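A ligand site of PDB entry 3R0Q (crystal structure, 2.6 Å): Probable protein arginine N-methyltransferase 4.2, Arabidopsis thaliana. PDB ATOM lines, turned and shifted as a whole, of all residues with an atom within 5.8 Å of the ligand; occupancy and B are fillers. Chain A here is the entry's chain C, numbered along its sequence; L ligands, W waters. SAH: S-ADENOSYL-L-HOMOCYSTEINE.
Water W2 lies within hydrogen-bond range of OG of Ser 74 (2.7 Å), OXT of the ligand (3.1 Å) and OE1 of Gln 38 (3.2 Å).
NH2 of Arg 47 lies within salt-bridge range of OXT of the ligand.
The backbone carbonyl oxygen (O) of Gly 71 is in hydrogen-bond range of a nitrogen (N) of the ligand.
OE2 of Glu 93 sits at hydrogen-bond distance from O2' of the ligand, at 2.7 Å.
The backbone NH (N) of Val 121 sits at hydrogen-bond distance from a nitrogen (N1) of the ligand (3.0 Å).
A nitrogen (N6) of the ligand lies within hydrogen-bond range of the side-chain hydroxyl of Ser 150.
A nitrogen (N6) of the ligand lies within hydrogen-bond range of the side-chain carboxylate (OE1) of Glu 122, at 3.2 Å.
NE2 of Gln 38 lies within hydrogen-bond range of O3' of the ligand (3.3 Å).
The backbone NH of Ala 94 sits at hydrogen-bond distance from a nitrogen (N3) of the ligand (3.3 Å).
A nitrogen (N) of the ligand sits at hydrogen-bond distance from the backbone carbonyl oxygen of Thr 72 (3.3 Å).
The side-chain hydroxyl (OG1) of Thr 95 sits at hydrogen-bond distance from an oxygen (O2') of the ligand, 3.5 Å away.
SD of Met 41 lies close to SD of the ligand (3.7 Å).
Residues that only touch the ligand: Ile 76 (3.3 Å), Met 147 (3.4 Å), Glu 136 (3.4 Å), Leu 77 (3.5 Å), Gly 119 (3.6 Å), Ser 120 (3.6 Å), Tyr 32 (3.6 Å), Phe 29 (3.8 Å), Gly 73 (3.8 Å), Tyr 28 (3.8 Å) and Val 92 (3.8 Å).
Hydrophobic or aromatic side chains within 4 Å of the ligand: Phe 29, Tyr 32, Met 41, Ile 76, Leu 77, Val 92, Ala 94, Val 121 and Met 147.
Within 4 Å of the ligand: Tyr 28, Phe 29, Tyr 32, Gln 38, Met 41, Arg 47, Gly 71, Thr 72, Gly 73, Ile 76, Leu 77, Val 92, Glu 93, Ala 94, Thr 95, Gly 119, Ser 120, Val 121, Glu 122, Glu 136, Met 147 and Ser 150.
The nearest printed residue that does not touch the ligand is Leu 42 (4.2 Å).
The guanidinium group (NH1) of Arg 47 is in salt-bridge range of the side-chain carboxylate (OE1) of Glu 136 (3.0 Å).
The backbone carbonyl oxygen of Val 92 lies within hydrogen-bond range of the backbone NH of Gly 71 (3.1 Å).
The side-chain carboxylate (OE1) of Glu 93 is in hydrogen-bond range of the backbone NH (N) of Gly 73, at 2.6 Å.
The side-chain hydroxyl (OG) of Ser 150 sits close to the side-chain carboxylate (OE2) of Glu 122 (3.2 Å).
The side-chain amide oxygen of Gln 38 sits close to the side-chain sulfur of Met 41 (3.6 Å).
The side-chain amide nitrogen of Gln 38 is in hydrogen-bond range of the backbone carbonyl oxygen of Tyr 32, at 2.8 Å.
OG1 of Thr 72 sits at hydrogen-bond distance from OD1 of Asp 69, 2.4 Å away.
The backbone NH (N) of Val 92 sits at hydrogen-bond distance from the backbone carbonyl oxygen (O) of Asp 69 (3.3 Å).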
ATOM      1  N   TYR A  28      -5.649 -29.908 -23.722  1.00  0.00           N
ATOM      2  CA  TYR A  28      -4.901 -29.229 -22.675  1.00  0.00           C
ATOM      3  C   TYR A  28      -4.379 -27.871 -23.138  1.00  0.00           C
ATOM      4  O   TYR A  28      -4.907 -26.828 -22.745  1.00  0.00           O
ATOM      5  CB  TYR A  28      -3.730 -30.105 -22.184  1.00  0.00           C
ATOM      6  CG  TYR A  28      -2.792 -29.343 -21.279  1.00  0.00           C
ATOM      7  CD1 TYR A  28      -3.207 -28.887 -20.035  1.00  0.00           C
ATOM      8  CD2 TYR A  28      -1.479 -29.074 -21.668  1.00  0.00           C
ATOM      9  CE1 TYR A  28      -2.351 -28.169 -19.207  1.00  0.00           C
ATOM     10  CE2 TYR A  28      -0.611 -28.363 -20.839  1.00  0.00           C
ATOM     11  CZ  TYR A  28      -1.058 -27.910 -19.613  1.00  0.00           C
ATOM     12  OH  TYR A  28      -0.208 -27.212 -18.777  1.00  0.00           O
ATOM     13  N   PHE A  29      -3.349 -27.873 -23.982  1.00  0.00           N
ATOM     14  CA  PHE A  29      -2.821 -26.625 -24.544  1.00  0.00           C
ATOM     15  C   PHE A  29      -3.962 -25.732 -25.048  1.00  0.00           C
ATOM     16  O   PHE A  29      -3.830 -24.509 -25.080  1.00  0.00           O
ATOM     17  CB  PHE A  29      -1.825 -26.900 -25.680  1.00  0.00           C
ATOM     18  CG  PHE A  29      -0.544 -27.538 -25.228  1.00  0.00           C
ATOM     19  CD1 PHE A  29      -0.037 -28.640 -25.883  1.00  0.00           C
ATOM     20  CD2 PHE A  29       0.160 -27.032 -24.145  1.00  0.00           C
ATOM     21  CE1 PHE A  29       1.152 -29.232 -25.466  1.00  0.00           C
ATOM     22  CE2 PHE A  29       1.337 -27.617 -23.730  1.00  0.00           C
ATOM     23  CZ  PHE A  29       1.832 -28.711 -24.387  1.00  0.00           C
ATOM     24  N   TYR A  32      -5.369 -22.829 -22.750  1.00  0.00           N
ATOM     25  CA  TYR A  32      -4.350 -21.859 -22.371  1.00  0.00           C
ATOM     26  C   TYR A  32      -4.057 -20.854 -23.483  1.00  0.00           C
ATOM     27  O   TYR A  32      -3.225 -19.969 -23.318  1.00  0.00           O
ATOM     28  CB  TYR A  32      -3.065 -22.570 -21.964  1.00  0.00           C
ATOM     29  CG  TYR A  32      -2.995 -22.930 -20.499  1.00  0.00           C
ATOM     30  CD1 TYR A  32      -3.183 -21.954 -19.523  1.00  0.00           C
ATOM     31  CD2 TYR A  32      -2.743 -24.225 -20.078  1.00  0.00           C
ATOM     32  CE1 TYR A  32      -3.121 -22.274 -18.176  1.00  0.00           C
ATOM     33  CE2 TYR A  32      -2.684 -24.554 -18.745  1.00  0.00           C
ATOM     34  CZ  TYR A  32      -2.865 -23.572 -17.797  1.00  0.00           C
ATOM     35  OH  TYR A  32      -2.808 -23.888 -16.458  1.00  0.00           O
ATOM     36  N   GLN A  38      -6.113 -16.572 -19.667  1.00  0.00           N
ATOM     37  CA  GLN A  38      -4.848 -16.049 -19.188  1.00  0.00           C
ATOM     38  C   GLN A  38      -5.042 -14.917 -18.194  1.00  0.00           C
ATOM     39  O   GLN A  38      -4.294 -14.814 -17.230  1.00  0.00           O
ATOM     40  CB  GLN A  38      -3.976 -15.600 -20.364  1.00  0.00           C
ATOM     41  CG  GLN A  38      -3.550 -16.746 -21.275  1.00  0.00           C
ATOM     42  CD  GLN A  38      -2.521 -17.675 -20.624  1.00  0.00           C
ATOM     43  OE1 GLN A  38      -2.355 -17.682 -19.408  1.00  0.00           O
ATOM     44  NE2 GLN A  38      -1.821 -18.437 -21.445  1.00  0.00           N
ATOM     45  N   MET A  41      -5.928 -16.059 -14.521  1.00  0.00           N
ATOM     46  CA  MET A  41      -4.723 -16.263 -13.728  1.00  0.00           C
ATOM     47  C   MET A  41      -4.125 -14.939 -13.268  1.00  0.00           C
ATOM     48  O   MET A  41      -3.816 -14.764 -12.085  1.00  0.00           O
ATOM     49  CB  MET A  41      -3.659 -17.014 -14.533  1.00  0.00           C
ATOM     50  CG  MET A  41      -4.135 -18.319 -15.116  1.00  0.00           C
ATOM     51  SD  MET A  41      -2.839 -19.038 -16.111  1.00  0.00           S
ATOM     52  CE  MET A  41      -2.138 -20.199 -14.945  1.00  0.00           C
ATOM     53  N   LEU A  42      -3.954 -14.022 -14.210  1.00  0.00           N
ATOM     54  CA  LEU A  42      -3.380 -12.720 -13.908  1.00  0.00           C
ATOM     55  C   LEU A  42      -4.232 -11.957 -12.896  1.00  0.00           C
ATOM     56  O   LEU A  42      -3.749 -10.998 -12.282  1.00  0.00           O
ATOM     57  CB  LEU A  42      -3.231 -11.908 -15.194  1.00  0.00           C
ATOM     58  CG  LEU A  42      -2.229 -12.433 -16.219  1.00  0.00           C
ATOM     59  CD1 LEU A  42      -2.520 -11.867 -17.593  1.00  0.00           C
ATOM     60  CD2 LEU A  42      -0.826 -12.077 -15.786  1.00  0.00           C
ATOM     61  N   ARG A  47      -1.811 -15.046  -6.148  1.00  0.00           N
ATOM     62  CA  ARG A  47      -0.834 -15.626  -7.065  1.00  0.00           C
ATOM     63  C   ARG A  47       0.176 -14.582  -7.547  1.00  0.00           C
ATOM     64  O   ARG A  47       1.385 -14.811  -7.501  1.00  0.00           O
ATOM     65  CB  ARG A  47      -1.542 -16.260  -8.261  1.00  0.00           C
ATOM     66  CG  ARG A  47      -0.645 -17.120  -9.126  1.00  0.00           C
ATOM     67  CD  ARG A  47      -1.322 -17.408 -10.441  1.00  0.00           C
ATOM     68  NE  ARG A  47      -0.979 -16.398 -11.420  1.00  0.00           N
ATOM     69  CZ  ARG A  47      -0.241 -16.644 -12.500  1.00  0.00           C
ATOM     70  NH1 ARG A  47       0.185 -17.870 -12.735  1.00  0.00           N
ATOM     71  NH2 ARG A  47       0.050 -15.672 -13.347  1.00  0.00           N
ATOM     72  N   MET A  48      -0.327 -13.425  -7.986  1.00  0.00           N
ATOM     73  CA  MET A  48       0.513 -12.369  -8.565  1.00  0.00           C
ATOM     74  C   MET A  48       1.478 -11.695  -7.587  1.00  0.00           C
ATOM     75  O   MET A  48       2.624 -11.404  -7.946  1.00  0.00           O
ATOM     76  CB  MET A  48      -0.378 -11.302  -9.239  1.00  0.00           C
ATOM     77  CG  MET A  48      -1.047 -11.760 -10.528  1.00  0.00           C
ATOM     78  SD  MET A  48       0.138 -11.999 -11.874  1.00  0.00           S
ATOM     79  CE  MET A  48      -0.215 -10.536 -12.830  1.00  0.00           C
ATOM     80  N   ASP A  69      11.999 -18.261 -18.685  1.00  0.00           N
ATOM     81  CA  ASP A  69      10.668 -18.355 -18.123  1.00  0.00           C
ATOM     82  C   ASP A  69       9.949 -19.521 -18.807  1.00  0.00           C
ATOM     83  O   ASP A  69       9.711 -19.482 -20.025  1.00  0.00           O
ATOM     84  CB  ASP A  69       9.913 -17.042 -18.357  1.00  0.00           C
ATOM     85  CG  ASP A  69       8.445 -17.146 -17.988  1.00  0.00           C
ATOM     86  OD1 ASP A  69       7.671 -16.281 -18.429  1.00  0.00           O
ATOM     87  OD2 ASP A  69       8.060 -18.083 -17.268  1.00  0.00           O
ATOM     88  N   VAL A  70       9.612 -20.547 -18.040  1.00  0.00           N
ATOM     89  CA  VAL A  70       9.012 -21.752 -18.615  1.00  0.00           C
ATOM     90  C   VAL A  70       7.489 -21.646 -18.693  1.00  0.00           C
ATOM     91  O   VAL A  70       6.803 -21.562 -17.675  1.00  0.00           O
ATOM     92  CB  VAL A  70       9.387 -23.017 -17.833  1.00  0.00           C
ATOM     93  CG1 VAL A  70       8.620 -24.201 -18.378  1.00  0.00           C
ATOM     94  CG2 VAL A  70      10.885 -23.261 -17.933  1.00  0.00           C
ATOM     95  N   GLY A  71       6.970 -21.643 -19.918  1.00  0.00           N
ATOM     96  CA  GLY A  71       5.533 -21.508 -20.118  1.00  0.00           C
ATOM     97  C   GLY A  71       5.087 -20.093 -19.805  1.00  0.00           C
ATOM     98  O   GLY A  71       4.344 -19.833 -18.855  1.00  0.00           O
ATOM     99  N   THR A  72       5.554 -19.171 -20.637  1.00  0.00           N
ATOM    100  CA  THR A  72       5.403 -17.749 -20.364  1.00  0.00           C
ATOM    101  C   THR A  72       3.963 -17.260 -20.530  1.00  0.00           C
ATOM    102  O   THR A  72       3.533 -16.335 -19.834  1.00  0.00           O
ATOM    103  CB  THR A  72       6.376 -16.929 -21.241  1.00  0.00           C
ATOM    104  OG1 THR A  72       6.733 -15.715 -20.578  1.00  0.00           O
ATOM    105  CG2 THR A  72       5.760 -16.644 -22.616  1.00  0.00           C
ATOM    106  N   GLY A  73       3.195 -17.879 -21.427  1.00  0.00           N
ATOM    107  CA  GLY A  73       1.831 -17.449 -21.681  1.00  0.00           C
ATOM    108  C   GLY A  73       1.810 -15.966 -22.026  1.00  0.00           C
ATOM    109  O   GLY A  73       2.398 -15.555 -23.031  1.00  0.00           O
ATOM    110  N   SER A  74       1.169 -15.159 -21.187  1.00  0.00           N
ATOM    111  CA  SER A  74       1.114 -13.715 -21.411  1.00  0.00           C
ATOM    112  C   SER A  74       2.501 -13.102 -21.431  1.00  0.00           C
ATOM    113  O   SER A  74       2.689 -11.973 -21.893  1.00  0.00           O
ATOM    114  CB  SER A  74       0.289 -13.039 -20.327  1.00  0.00           C
ATOM    115  OG  SER A  74       0.939 -13.123 -19.082  1.00  0.00           O
ATOM    116  N   GLY A  75       3.474 -13.844 -20.920  1.00  0.00           N
ATOM    117  CA  GLY A  75       4.818 -13.322 -20.746  1.00  0.00           C
ATOM    118  C   GLY A  75       4.942 -12.434 -19.531  1.00  0.00           C
ATOM    119  O   GLY A  75       5.857 -11.624 -19.451  1.00  0.00           O
ATOM    120  N   ILE A  76       4.025 -12.560 -18.573  1.00  0.00           N
ATOM    121  CA  ILE A  76       4.073 -11.707 -17.386  1.00  0.00           C
ATOM    122  C   ILE A  76       5.340 -11.890 -16.524  1.00  0.00           C
ATOM    123  O   ILE A  76       6.022 -10.912 -16.210  1.00  0.00           O
ATOM    124  CB  ILE A  76       2.804 -11.828 -16.509  1.00  0.00           C
ATOM    125  CG1 ILE A  76       2.759 -10.671 -15.516  1.00  0.00           C
ATOM    126  CG2 ILE A  76       2.746 -13.155 -15.770  1.00  0.00           C
ATOM    127  CD1 ILE A  76       2.842  -9.312 -16.183  1.00  0.00           C
ATOM    128  N   LEU A  77       5.662 -13.122 -16.150  1.00  0.00           N
ATOM    129  CA  LEU A  77       6.825 -13.381 -15.301  1.00  0.00           C
ATOM    130  C   LEU A  77       8.109 -13.012 -16.036  1.00  0.00           C
ATOM    131  O   LEU A  77       9.101 -12.624 -15.406  1.00  0.00           O
ATOM    132  CB  LEU A  77       6.852 -14.855 -14.843  1.00  0.00           C
ATOM    133  CG  LEU A  77       5.563 -15.410 -14.231  1.00  0.00           C
ATOM    134  CD1 LEU A  77       5.738 -16.846 -13.767  1.00  0.00           C
ATOM    135  CD2 LEU A  77       5.055 -14.531 -13.084  1.00  0.00           C
ATOM    136  N   VAL A  92       9.473 -18.972 -23.278  1.00  0.00           N
ATOM    137  CA  VAL A  92       9.015 -20.077 -24.109  1.00  0.00           C
ATOM    138  C   VAL A  92       7.504 -20.307 -23.914  1.00  0.00           C
ATOM    139  O   VAL A  92       7.052 -20.497 -22.795  1.00  0.00           O
ATOM    140  CB  VAL A  92       9.800 -21.361 -23.731  1.00  0.00           C
ATOM    141  CG1 VAL A  92       9.210 -22.608 -24.381  1.00  0.00           C
ATOM    142  CG2 VAL A  92      11.270 -21.200 -24.104  1.00  0.00           C
ATOM    143  N   GLU A  93       6.735 -20.256 -25.005  1.00  0.00           N
ATOM    144  CA  GLU A  93       5.290 -20.527 -24.922  1.00  0.00           C
ATOM    145  C   GLU A  93       4.851 -21.456 -26.047  1.00  0.00           C
ATOM    146  O   GLU A  93       5.135 -21.209 -27.209  1.00  0.00           O
ATOM    147  CB  GLU A  93       4.476 -19.225 -24.969  1.00  0.00           C
ATOM    148  CG  GLU A  93       2.973 -19.414 -25.168  1.00  0.00           C
ATOM    149  CD  GLU A  93       2.319 -20.232 -24.057  1.00  0.00           C
ATOM    150  OE1 GLU A  93       2.654 -20.014 -22.874  1.00  0.00           O
ATOM    151  OE2 GLU A  93       1.467 -21.092 -24.376  1.00  0.00           O
ATOM    152  N   ALA A  94       4.134 -22.517 -25.689  1.00  0.00           N
ATOM    153  CA  ALA A  94       3.778 -23.556 -26.648  1.00  0.00           C
ATOM    154  C   ALA A  94       2.625 -23.150 -27.570  1.00  0.00           C
ATOM    155  O   ALA A  94       2.436 -23.716 -28.650  1.00  0.00           O
ATOM    156  CB  ALA A  94       3.445 -24.855 -25.920  1.00  0.00           C
ATOM    157  N   THR A  95       1.846 -22.152 -27.144  1.00  0.00           N
ATOM    158  CA  THR A  95       0.622 -21.761 -27.822  1.00  0.00           C
ATOM    159  C   THR A  95       0.792 -20.479 -28.653  1.00  0.00           C
ATOM    160  O   THR A  95       1.835 -19.819 -28.592  1.00  0.00           O
ATOM    161  CB  THR A  95      -0.510 -21.531 -26.805  1.00  0.00           C
ATOM    162  OG1 THR A  95      -0.518 -22.583 -25.837  1.00  0.00           O
ATOM    163  CG2 THR A  95      -1.842 -21.520 -27.491  1.00  0.00           C
ATOM    164  N   MET A  97      -0.405 -17.976 -27.960  1.00  0.00           N
ATOM    165  CA  MET A  97      -0.352 -16.939 -26.940  1.00  0.00           C
ATOM    166  C   MET A  97       1.014 -16.266 -27.024  1.00  0.00           C
ATOM    167  O   MET A  97       1.190 -15.153 -26.574  1.00  0.00           O
ATOM    168  CB  MET A  97      -0.549 -17.545 -25.552  1.00  0.00           C
ATOM    169  CG  MET A  97      -0.809 -16.514 -24.481  1.00  0.00           C
ATOM    170  SD  MET A  97      -2.457 -15.790 -24.593  1.00  0.00           S
ATOM    171  CE  MET A  97      -2.109 -14.159 -23.931  1.00  0.00           C
ATOM    172  N   GLY A 119       6.634 -22.560 -29.088  1.00  0.00           N
ATOM    173  CA  GLY A 119       6.993 -23.957 -29.247  1.00  0.00           C
ATOM    174  C   GLY A 119       7.093 -24.664 -27.906  1.00  0.00           C
ATOM    175  O   GLY A 119       7.169 -24.028 -26.850  1.00  0.00           O
ATOM    176  N   SER A 120       7.093 -25.980 -27.960  1.00  0.00           N
ATOM    177  CA  SER A 120       7.085 -26.786 -26.752  1.00  0.00           C
ATOM    178  C   SER A 120       8.497 -26.941 -26.190  1.00  0.00           C
ATOM    179  O   SER A 120       9.343 -27.581 -26.818  1.00  0.00           O
ATOM    180  CB  SER A 120       6.470 -28.157 -27.068  1.00  0.00           C
ATOM    181  OG  SER A 120       6.057 -28.830 -25.905  1.00  0.00           O
ATOM    182  N   VAL A 121       8.745 -26.364 -25.019  1.00  0.00           N
ATOM    183  CA  VAL A 121      10.085 -26.368 -24.411  1.00  0.00           C
ATOM    184  C   VAL A 121      10.844 -27.683 -24.611  1.00  0.00           C
ATOM    185  O   VAL A 121      12.064 -27.708 -24.642  1.00  0.00           O
ATOM    186  CB  VAL A 121      10.045 -26.013 -22.900  1.00  0.00           C
ATOM    187  CG1 VAL A 121       9.855 -27.259 -22.066  1.00  0.00           C
ATOM    188  CG2 VAL A 121      11.326 -25.276 -22.483  1.00  0.00           C
ATOM    189  N   GLU A 122      10.104 -28.778 -24.746  1.00  0.00           N
ATOM    190  CA  GLU A 122      10.747 -30.057 -24.968  1.00  0.00           C
ATOM    191  C   GLU A 122      11.460 -30.110 -26.320  1.00  0.00           C
ATOM    192  O   GLU A 122      12.339 -30.947 -26.518  1.00  0.00           O
ATOM    193  CB  GLU A 122       9.727 -31.189 -24.895  1.00  0.00           C
ATOM    194  CG  GLU A 122       9.465 -31.685 -23.507  1.00  0.00           C
ATOM    195  CD  GLU A 122       8.527 -30.800 -22.769  1.00  0.00           C
ATOM    196  OE1 GLU A 122       7.421 -30.540 -23.262  1.00  0.00           O
ATOM    197  OE2 GLU A 122       8.901 -30.336 -21.677  1.00  0.00           O
ATOM    198  N   GLU A 136       5.544 -20.981 -13.523  1.00  0.00           N
ATOM    199  CA  GLU A 136       4.398 -21.130 -12.689  1.00  0.00           C
ATOM    200  C   GLU A 136       3.649 -22.361 -13.214  1.00  0.00           C
ATOM    201  O   GLU A 136       2.771 -22.266 -14.063  1.00  0.00           O
ATOM    202  CB  GLU A 136       3.526 -19.864 -12.725  1.00  0.00           C
ATOM    203  CG  GLU A 136       2.433 -19.846 -11.668  1.00  0.00           C
ATOM    204  CD  GLU A 136       1.223 -20.638 -12.116  1.00  0.00           C
ATOM    205  OE1 GLU A 136       0.994 -20.733 -13.332  1.00  0.00           O
ATOM    206  OE2 GLU A 136       0.490 -21.172 -11.268  1.00  0.00           O
ATOM    207  N   MET A 147       2.720 -30.322 -15.736  1.00  0.00           N
ATOM    208  CA  MET A 147       3.540 -29.336 -16.420  1.00  0.00           C
ATOM    209  C   MET A 147       4.939 -29.213 -15.800  1.00  0.00           C
ATOM    210  O   MET A 147       5.860 -28.689 -16.434  1.00  0.00           O
ATOM    211  CB  MET A 147       2.852 -27.971 -16.436  1.00  0.00           C
ATOM    212  CG  MET A 147       3.673 -26.892 -17.133  1.00  0.00           C
ATOM    213  SD  MET A 147       3.024 -25.233 -16.866  1.00  0.00           S
ATOM    214  CE  MET A 147       4.415 -24.248 -17.395  1.00  0.00           C
ATOM    215  N   SER A 150       7.782 -30.606 -17.759  1.00  0.00           N
ATOM    216  CA  SER A 150       8.377 -29.787 -18.805  1.00  0.00           C
ATOM    217  C   SER A 150       9.505 -28.979 -18.196  1.00  0.00           C
ATOM    218  O   SER A 150      10.569 -28.825 -18.797  1.00  0.00           O
ATOM    219  CB  SER A 150       7.325 -28.856 -19.416  1.00  0.00           C
ATOM    220  OG  SER A 150       6.287 -29.602 -20.033  1.00  0.00           O
ATOM    221  N   ARG A 348      -1.827 -36.625 -17.462  1.00  0.00           N
ATOM    222  CA  ARG A 348      -1.974 -35.322 -16.810  1.00  0.00           C
ATOM    223  C   ARG A 348      -3.059 -35.298 -15.731  1.00  0.00           C
ATOM    224  O   ARG A 348      -3.177 -34.343 -14.975  1.00  0.00           O
ATOM    225  CB  ARG A 348      -2.245 -34.204 -17.834  1.00  0.00           C
ATOM    226  CG  ARG A 348      -1.046 -33.840 -18.692  1.00  0.00           C
ATOM    227  CD  ARG A 348      -1.356 -32.721 -19.677  1.00  0.00           C
ATOM    228  NE  ARG A 348      -0.283 -32.550 -20.657  1.00  0.00           N
ATOM    229  CZ  ARG A 348       0.711 -31.671 -20.538  1.00  0.00           C
ATOM    230  NH1 ARG A 348       0.758 -30.865 -19.482  1.00  0.00           N
ATOM    231  NH2 ARG A 348       1.651 -31.583 -21.476  1.00  0.00           N
HETATM  232  N   SAH L   1       3.471 -18.058 -17.001  1.00  0.00           N
HETATM  233  CA  SAH L   1       2.152 -17.443 -17.021  1.00  0.00           C
HETATM  234  CB  SAH L   1       1.077 -18.472 -17.324  1.00  0.00           C
HETATM  235  CG  SAH L   1       1.305 -19.787 -16.605  1.00  0.00           C
HETATM  236  SD  SAH L   1       0.085 -21.009 -17.132  1.00  0.00           S
HETATM  237  C   SAH L   1       1.805 -16.816 -15.689  1.00  0.00           C
HETATM  238  O   SAH L   1       2.333 -17.213 -14.643  1.00  0.00           O
HETATM  239  OXT SAH L   1       0.966 -15.910 -15.641  1.00  0.00           O
HETATM  240  C5' SAH L   1       1.354 -22.029 -17.903  1.00  0.00           C
HETATM  241  C4' SAH L   1       1.650 -21.742 -19.373  1.00  0.00           C
HETATM  242  O4' SAH L   1       2.725 -22.571 -19.786  1.00  0.00           O
HETATM  243  C3' SAH L   1       0.494 -22.028 -20.334  1.00  0.00           C
HETATM  244  O3' SAH L   1       0.308 -20.880 -21.122  1.00  0.00           O
HETATM  245  C2' SAH L   1       0.953 -23.182 -21.219  1.00  0.00           C
HETATM  246  O2' SAH L   1       0.637 -22.976 -22.571  1.00  0.00           O
HETATM  247  C1' SAH L   1       2.458 -23.148 -21.059  1.00  0.00           C
HETATM  248  N9  SAH L   1       3.097 -24.459 -21.165  1.00  0.00           N
HETATM  249  C8  SAH L   1       2.794 -25.635 -20.520  1.00  0.00           C
HETATM  250  N7  SAH L   1       3.678 -26.581 -20.931  1.00  0.00           N
HETATM  251  C5  SAH L   1       4.531 -26.027 -21.825  1.00  0.00           C
HETATM  252  C6  SAH L   1       5.611 -26.518 -22.559  1.00  0.00           C
HETATM  253  N6  SAH L   1       6.016 -27.779 -22.466  1.00  0.00           N
HETATM  254  N1  SAH L   1       6.291 -25.658 -23.392  1.00  0.00           N
HETATM  255  C2  SAH L   1       5.898 -24.346 -23.523  1.00  0.00           C
HETATM  256  N3  SAH L   1       4.832 -23.875 -22.793  1.00  0.00           N
HETATM  257  C4  SAH L   1       4.172 -24.701 -21.960  1.00  0.00           C
HETATM  258  O   HOH W   1       5.713 -19.677 -16.102  1.00  0.00           O
HETATM  259  O   HOH W   2      -0.185 -15.555 -18.469  1.00  0.00           O
